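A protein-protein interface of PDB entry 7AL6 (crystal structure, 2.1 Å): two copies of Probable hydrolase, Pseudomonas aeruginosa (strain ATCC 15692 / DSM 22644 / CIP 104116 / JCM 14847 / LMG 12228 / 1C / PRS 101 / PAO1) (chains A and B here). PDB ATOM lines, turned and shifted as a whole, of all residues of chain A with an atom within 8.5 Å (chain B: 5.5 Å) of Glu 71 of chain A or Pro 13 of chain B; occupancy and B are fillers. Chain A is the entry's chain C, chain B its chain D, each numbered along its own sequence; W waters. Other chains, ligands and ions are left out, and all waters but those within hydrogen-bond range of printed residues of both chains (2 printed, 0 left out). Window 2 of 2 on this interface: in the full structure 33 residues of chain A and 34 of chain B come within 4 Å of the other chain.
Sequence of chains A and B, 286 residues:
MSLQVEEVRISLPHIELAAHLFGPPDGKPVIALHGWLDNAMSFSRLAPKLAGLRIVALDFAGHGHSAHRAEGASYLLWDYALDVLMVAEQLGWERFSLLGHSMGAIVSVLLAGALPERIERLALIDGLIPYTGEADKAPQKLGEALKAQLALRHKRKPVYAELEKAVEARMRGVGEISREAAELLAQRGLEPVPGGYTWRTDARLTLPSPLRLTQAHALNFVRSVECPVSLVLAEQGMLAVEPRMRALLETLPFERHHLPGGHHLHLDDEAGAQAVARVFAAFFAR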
ATOM      1  N   HIS A  68     -28.306  -6.726  20.329  1.00  0.00           N
ATOM      2  CA  HIS A  68     -27.221  -7.395  21.022  1.00  0.00           C
ATOM      3  C   HIS A  68     -27.375  -7.089  22.490  1.00  0.00           C
ATOM      4  O   HIS A  68     -27.875  -6.027  22.859  1.00  0.00           O
ATOM      5  CB  HIS A  68     -25.841  -6.888  20.539  1.00  0.00           C
ATOM      6  CG  HIS A  68     -25.566  -7.141  19.105  1.00  0.00           C
ATOM      7  ND1 HIS A  68     -25.597  -8.407  18.541  1.00  0.00           N
ATOM      8  CD2 HIS A  68     -25.189  -6.294  18.119  1.00  0.00           C
ATOM      9  CE1 HIS A  68     -25.284  -8.314  17.260  1.00  0.00           C
ATOM     10  NE2 HIS A  68     -25.011  -7.048  16.986  1.00  0.00           N
ATOM     11  N   ARG A  69     -26.922  -8.001  23.351  1.00  0.00           N
ATOM     12  CA  ARG A  69     -27.005  -7.693  24.777  1.00  0.00           C
ATOM     13  C   ARG A  69     -26.043  -6.557  25.124  1.00  0.00           C
ATOM     14  O   ARG A  69     -25.072  -6.324  24.423  1.00  0.00           O
ATOM     15  CB  ARG A  69     -26.639  -8.903  25.642  1.00  0.00           C
ATOM     16  CG  ARG A  69     -27.571 -10.127  25.445  1.00  0.00           C
ATOM     17  CD  ARG A  69     -27.472 -11.068  26.596  1.00  0.00           C
ATOM     18  NE  ARG A  69     -28.158 -12.347  26.333  1.00  0.00           N
ATOM     19  CZ  ARG A  69     -29.482 -12.519  26.355  1.00  0.00           C
ATOM     20  NH1 ARG A  69     -30.275 -11.488  26.596  1.00  0.00           N
ATOM     21  NH2 ARG A  69     -30.008 -13.730  26.137  1.00  0.00           N
ATOM     22  N   ALA A  70     -26.301  -5.894  26.245  1.00  0.00           N
ATOM     23  CA  ALA A  70     -25.433  -4.843  26.761  1.00  0.00           C
ATOM     24  C   ALA A  70     -24.053  -5.400  27.126  1.00  0.00           C
ATOM     25  O   ALA A  70     -23.834  -6.613  27.248  1.00  0.00           O
ATOM     26  CB  ALA A  70     -26.070  -4.191  27.985  1.00  0.00           C
ATOM     27  N   GLU A  71     -23.105  -4.499  27.285  1.00  0.00           N
ATOM     28  CA  GLU A  71     -21.705  -4.881  27.538  1.00  0.00           C
ATOM     29  C   GLU A  71     -21.623  -5.658  28.853  1.00  0.00           C
ATOM     30  O   GLU A  71     -22.252  -5.290  29.811  1.00  0.00           O
ATOM     31  CB  GLU A  71     -20.796  -3.652  27.440  1.00  0.00           C
ATOM     32  CG  GLU A  71     -20.665  -2.840  28.706  1.00  0.00           C
ATOM     33  CD  GLU A  71     -19.548  -1.797  28.675  1.00  0.00           C
ATOM     34  OE1 GLU A  71     -19.646  -0.773  29.379  1.00  0.00           O
ATOM     35  OE2 GLU A  71     -18.571  -2.011  27.938  1.00  0.00           O
ATOM     36  N   GLY A  72     -20.908  -6.764  28.810  1.00  0.00           N
ATOM     37  CA  GLY A  72     -20.619  -7.602  29.959  1.00  0.00           C
ATOM     38  C   GLY A  72     -21.624  -8.706  30.174  1.00  0.00           C
ATOM     39  O   GLY A  72     -21.389  -9.584  31.009  1.00  0.00           O
ATOM     40  N   ALA A  73     -22.734  -8.692  29.442  1.00  0.00           N
ATOM     41  CA  ALA A  73     -23.773  -9.694  29.632  1.00  0.00           C
ATOM     42  C   ALA A  73     -23.446 -10.956  28.842  1.00  0.00           C
ATOM     43  O   ALA A  73     -22.760 -10.925  27.822  1.00  0.00           O
ATOM     44  CB  ALA A  73     -25.129  -9.169  29.181  1.00  0.00           C
ATOM     45  N   SER A  74     -23.962 -12.069  29.298  1.00  0.00           N
ATOM     46  CA  SER A  74     -23.657 -13.397  28.746  1.00  0.00           C
ATOM     47  C   SER A  74     -24.744 -13.912  27.807  1.00  0.00           C
ATOM     48  O   SER A  74     -25.829 -13.433  27.846  1.00  0.00           O
ATOM     49  CB  SER A  74     -23.417 -14.312  29.884  1.00  0.00           C
ATOM     50  OG  SER A  74     -24.574 -14.451  30.660  1.00  0.00           O
ATOM     51  N   TYR A  75     -24.412 -14.899  27.004  1.00  0.00           N
ATOM     52  CA  TYR A  75     -25.356 -15.562  26.090  1.00  0.00           C
ATOM     53  C   TYR A  75     -25.468 -17.031  26.502  1.00  0.00           C
ATOM     54  O   TYR A  75     -25.196 -17.861  25.707  1.00  0.00           O
ATOM     55  CB  TYR A  75     -24.926 -15.420  24.637  1.00  0.00           C
ATOM     56  CG  TYR A  75     -25.124 -14.060  24.022  1.00  0.00           C
ATOM     57  CD1 TYR A  75     -26.291 -13.733  23.358  1.00  0.00           C
ATOM     58  CD2 TYR A  75     -24.129 -13.107  24.068  1.00  0.00           C
ATOM     59  CE1 TYR A  75     -26.460 -12.501  22.757  1.00  0.00           C
ATOM     60  CE2 TYR A  75     -24.278 -11.872  23.464  1.00  0.00           C
ATOM     61  CZ  TYR A  75     -25.450 -11.563  22.808  1.00  0.00           C
ATOM     62  OH  TYR A  75     -25.602 -10.356  22.227  1.00  0.00           O
ATOM     63  N   GLN A 149     -12.629 -15.072  27.243  1.00  0.00           N
ATOM     64  CA  GLN A 149     -13.141 -13.733  27.522  1.00  0.00           C
ATOM     65  C   GLN A 149     -12.038 -12.696  27.446  1.00  0.00           C
ATOM     66  O   GLN A 149     -12.196 -11.655  26.807  1.00  0.00           O
ATOM     67  CB  GLN A 149     -13.794 -13.705  28.912  1.00  0.00           C
ATOM     68  CG  GLN A 149     -15.131 -14.387  28.952  1.00  0.00           C
ATOM     69  CD  GLN A 149     -16.310 -13.417  28.897  1.00  0.00           C
ATOM     70  OE1 GLN A 149     -16.219 -12.300  28.362  1.00  0.00           O
ATOM     71  NE2 GLN A 149     -17.423 -13.843  29.482  1.00  0.00           N
ATOM     72  N   LEU A 150     -10.894 -12.987  28.064  1.00  0.00           N
ATOM     73  CA  LEU A 150      -9.752 -12.076  28.024  1.00  0.00           C
ATOM     74  C   LEU A 150      -9.239 -11.862  26.608  1.00  0.00           C
ATOM     75  O   LEU A 150      -8.747 -10.780  26.282  1.00  0.00           O
ATOM     76  CB  LEU A 150      -8.622 -12.635  28.885  1.00  0.00           C
ATOM     77  CG  LEU A 150      -8.795 -12.605  30.401  1.00  0.00           C
ATOM     78  CD1 LEU A 150      -7.537 -13.282  30.995  1.00  0.00           C
ATOM     79  CD2 LEU A 150      -8.966 -11.202  30.976  1.00  0.00           C
ATOM     80  N   LEU A 152     -11.034 -12.068  23.758  1.00  0.00           N
ATOM     81  CA  LEU A 152     -12.036 -11.701  22.770  1.00  0.00           C
ATOM     82  C   LEU A 152     -11.711 -10.312  22.236  1.00  0.00           C
ATOM     83  O   LEU A 152     -11.322  -9.419  22.990  1.00  0.00           O
ATOM     84  CB  LEU A 152     -13.433 -11.739  23.391  1.00  0.00           C
ATOM     85  CG  LEU A 152     -14.593 -11.835  22.393  1.00  0.00           C
ATOM     86  CD1 LEU A 152     -14.564 -13.137  21.606  1.00  0.00           C
ATOM     87  CD2 LEU A 152     -15.934 -11.664  23.122  1.00  0.00           C
ATOM     88  N   ARG A 153     -11.835 -10.140  20.924  1.00  0.00           N
ATOM     89  CA  ARG A 153     -11.362  -8.917  20.290  1.00  0.00           C
ATOM     90  C   ARG A 153     -12.337  -8.401  19.239  1.00  0.00           C
ATOM     91  O   ARG A 153     -13.108  -9.161  18.642  1.00  0.00           O
ATOM     92  CB  ARG A 153     -10.000  -9.126  19.620  1.00  0.00           C
ATOM     93  CG  ARG A 153      -8.835  -9.172  20.570  1.00  0.00           C
ATOM     94  CD  ARG A 153      -8.680  -7.910  21.447  1.00  0.00           C
ATOM     95  NE  ARG A 153      -7.428  -8.028  22.199  1.00  0.00           N
ATOM     96  CZ  ARG A 153      -7.331  -8.499  23.443  1.00  0.00           C
ATOM     97  NH1 ARG A 153      -8.424  -8.857  24.109  1.00  0.00           N
ATOM     98  NH2 ARG A 153      -6.140  -8.602  24.030  1.00  0.00           N
ATOM     99  N   ASP A 202     -22.932 -11.402  17.231  1.00  0.00           N
ATOM    100  CA  ASP A 202     -22.191 -10.890  18.365  1.00  0.00           C
ATOM    101  C   ASP A 202     -21.008 -11.830  18.586  1.00  0.00           C
ATOM    102  O   ASP A 202     -21.164 -13.061  18.651  1.00  0.00           O
ATOM    103  CB  ASP A 202     -23.148 -10.802  19.555  1.00  0.00           C
ATOM    104  CG  ASP A 202     -22.591 -10.058  20.734  1.00  0.00           C
ATOM    105  OD1 ASP A 202     -21.397 -10.253  21.064  1.00  0.00           O
ATOM    106  OD2 ASP A 202     -23.392  -9.348  21.401  1.00  0.00           O
ATOM    107  N   ARG A 204     -19.503 -12.404  21.195  1.00  0.00           N
ATOM    108  CA  ARG A 204     -19.559 -13.176  22.432  1.00  0.00           C
ATOM    109  C   ARG A 204     -20.308 -14.494  22.269  1.00  0.00           C
ATOM    110  O   ARG A 204     -20.248 -15.337  23.169  1.00  0.00           O
ATOM    111  CB  ARG A 204     -20.202 -12.351  23.532  1.00  0.00           C
ATOM    112  CG  ARG A 204     -19.466 -11.063  23.834  1.00  0.00           C
ATOM    113  CD  ARG A 204     -20.316 -10.267  24.828  1.00  0.00           C
ATOM    114  NE  ARG A 204     -21.232  -9.433  24.063  1.00  0.00           N
ATOM    115  CZ  ARG A 204     -22.129  -8.608  24.586  1.00  0.00           C
ATOM    116  NH1 ARG A 204     -22.287  -8.540  25.901  1.00  0.00           N
ATOM    117  NH2 ARG A 204     -22.879  -7.862  23.780  1.00  0.00           N
ATOM    118  N   SER B  11     -10.708   1.054  34.637  1.00  0.00           N
ATOM    119  CA  SER B  11     -11.595   0.907  33.485  1.00  0.00           C
ATOM    120  C   SER B  11     -11.348  -0.449  32.839  1.00  0.00           C
ATOM    121  O   SER B  11     -10.268  -0.702  32.297  1.00  0.00           O
ATOM    122  CB  SER B  11     -11.367   2.026  32.468  1.00  0.00           C
ATOM    123  OG  SER B  11     -11.717   3.287  33.013  1.00  0.00           O
ATOM    124  N   LEU B  12     -12.334  -1.320  32.915  1.00  0.00           N
ATOM    125  CA  LEU B  12     -12.365  -2.564  32.168  1.00  0.00           C
ATOM    126  C   LEU B  12     -13.221  -2.398  30.929  1.00  0.00           C
ATOM    127  O   LEU B  12     -13.982  -1.438  30.794  1.00  0.00           O
ATOM    128  CB  LEU B  12     -12.919  -3.700  33.038  1.00  0.00           C
ATOM    129  CG  LEU B  12     -12.363  -3.778  34.432  1.00  0.00           C
ATOM    130  CD1 LEU B  12     -12.880  -5.000  35.158  1.00  0.00           C
ATOM    131  CD2 LEU B  12     -10.849  -3.744  34.332  1.00  0.00           C
ATOM    132  N   PRO B  13     -13.131  -3.333  29.997  1.00  0.00           N
ATOM    133  CA  PRO B  13     -13.892  -3.173  28.752  1.00  0.00           C
ATOM    134  C   PRO B  13     -15.373  -3.023  28.979  1.00  0.00           C
ATOM    135  O   PRO B  13     -16.036  -2.319  28.226  1.00  0.00           O
ATOM    136  CB  PRO B  13     -13.554  -4.446  27.967  1.00  0.00           C
ATOM    137  CG  PRO B  13     -12.212  -4.899  28.525  1.00  0.00           C
ATOM    138  CD  PRO B  13     -12.227  -4.496  29.991  1.00  0.00           C
ATOM    139  N   HIS B  14     -15.918  -3.639  30.021  1.00  0.00           N
ATOM    140  CA  HIS B  14     -17.355  -3.715  30.211  1.00  0.00           C
ATOM    141  C   HIS B  14     -17.823  -2.946  31.447  1.00  0.00           C
ATOM    142  O   HIS B  14     -19.053  -2.795  31.598  1.00  0.00           O
ATOM    143  CB  HIS B  14     -17.797  -5.183  30.363  1.00  0.00           C
ATOM    144  CG  HIS B  14     -17.104  -5.915  31.479  1.00  0.00           C
ATOM    145  ND1 HIS B  14     -15.743  -6.151  31.483  1.00  0.00           N
ATOM    146  CD2 HIS B  14     -17.585  -6.454  32.631  1.00  0.00           C
ATOM    147  CE1 HIS B  14     -15.426  -6.816  32.582  1.00  0.00           C
ATOM    148  NE2 HIS B  14     -16.526  -7.025  33.287  1.00  0.00           N
ATOM    149  N   ILE B  15     -16.952  -2.494  32.283  1.00  0.00           N
ATOM    150  CA  ILE B  15     -17.342  -1.898  33.561  1.00  0.00           C
ATOM    151  C   ILE B  15     -16.175  -1.149  34.164  1.00  0.00           C
ATOM    152  O   ILE B  15     -14.992  -1.465  33.883  1.00  0.00           O
ATOM    153  CB  ILE B  15     -17.869  -3.031  34.496  1.00  0.00           C
ATOM    154  CG1 ILE B  15     -18.687  -2.443  35.628  1.00  0.00           C
ATOM    155  CG2 ILE B  15     -16.736  -3.878  35.025  1.00  0.00           C
ATOM    156  CD1 ILE B  15     -19.363  -3.519  36.425  1.00  0.00           C
ATOM    157  N   ALA B  70     -24.088  -3.342  33.579  1.00  0.00           N
ATOM    158  CA  ALA B  70     -25.088  -2.941  32.616  1.00  0.00           C
ATOM    159  C   ALA B  70     -26.332  -3.828  32.713  1.00  0.00           C
ATOM    160  O   ALA B  70     -26.342  -4.892  33.333  1.00  0.00           O
ATOM    161  CB  ALA B  70     -24.502  -2.985  31.205  1.00  0.00           C
ATOM    162  N   ALA B  73     -27.003  -7.947  32.703  1.00  0.00           N
ATOM    163  CA  ALA B  73     -25.853  -8.722  33.128  1.00  0.00           C
ATOM    164  C   ALA B  73     -26.109  -9.336  34.507  1.00  0.00           C
ATOM    165  O   ALA B  73     -26.825  -8.775  35.339  1.00  0.00           O
ATOM    166  CB  ALA B  73     -24.598  -7.844  33.175  1.00  0.00           C
ATOM    167  N   MET B  86      -9.434  -9.215  34.829  1.00  0.00           N
ATOM    168  CA  MET B  86      -9.281  -8.022  34.004  1.00  0.00           C
ATOM    169  C   MET B  86      -8.699  -6.866  34.787  1.00  0.00           C
ATOM    170  O   MET B  86      -8.032  -6.001  34.199  1.00  0.00           O
ATOM    171  CB  MET B  86     -10.625  -7.660  33.412  1.00  0.00           C
ATOM    172  CG  MET B  86     -10.944  -8.517  32.248  1.00  0.00           C
ATOM    173  SD  MET B  86     -12.608  -8.142  31.615  1.00  0.00           S
ATOM    174  CE  MET B  86     -12.394  -8.894  30.011  1.00  0.00           C
HETATM  175  O   HOH W   1     -21.691  -4.664  32.371  1.00  0.00           O
HETATM  176  O   HOH W   2     -21.395  -1.050  31.427  1.00  0.00           O
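The side-chain sulfur (SD) of Met 86 of chain B sits close to a ring nitrogen (ND1) of His 14 of chain B (3.7 Å). NH1 of Arg 204 of chain A is in hydrogen-bond range of O of Ala 70 of chain A (2.8 Å). The backbone carbonyl oxygen of Leu 150 of chain A lies within hydrogen-bond range of the guanidinium group of Arg 153 of chain A.
Of the 14 printed residues of chain A, 4 touch a printed residue of chain B. Hydrophobic or aromatic side chains of chain A within 4 Å of the printed part of chain B: Ala 70 and Leu 150. Hydrophobic or aromatic side chains of chain B that line the printed part of chain A: His 14, Ala 70 and Met 86. Among the printed residues, no Asp or Glu carboxylate lies within 4 Å of a Lys or Arg side-chain nitrogen of the other chain.
Glu 71 of chain A touches just these residues of chain B: Pro 13, His 14 and Ala 70. Of chain A, only Glu 71 comes within 4 Å of Pro 13 of chain B. Printed residues of chain A within 4 Å of His 14 of chain B: Glu 71 (3.1 Å) and Gly 72 (3.7 Å). Of the printed residues of chain B, Leu 150 of chain A touches Met 86. Ile 15 of chain B touches none of the printed residues of chain A. The nearest residue of chain B that does not touch Glu 71 of chain A is Ile 15 of chain B (4.3 Å). The nearest printed residue of chain B that does not touch Leu 150 of chain A is Pro 13 of chain B (7.2 Å).
Water W1 lies within hydrogen-bond range of O of Glu 71 of chain A (2.7 Å), N of Ala 70 of chain B (3.0 Å) and O of His 14 of chain B (3.3 Å). Water W2 lies within hydrogen-bond range of the side-chain carboxylate of Glu 71 of chain A (2.7 Å) and the backbone carbonyl oxygen of His 14 of chain B (2.9 Å).
CB of Ala 70 of chain A touches CB of Ala 70 of chain B, at 3.8 Å. Glu 71 of chain A touches Ala 70 of chain B. Gly 72 of chain A touches His 14 of chain B (CA to CB, 3.7 Å). Leu 150 of chain A touches Met 86 of chain B (CD2 to CG, 3.6 Å).
The side-chain carboxylate (OE1) of Glu 71 of chain A lies close to the backbone carbonyl oxygen (O) of His 14 of chain B, 3.1 Å away. OE2 of Glu 71 of chain A sits close to O of Pro 13 of chain B (2.6 Å).
Ala 70 of chain A touches its own counterpart, Ala 70 of chain B. Of the 6 pairs that touch across the chains among the printed residues, 1 has its exchanged pair printed and touching as well.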
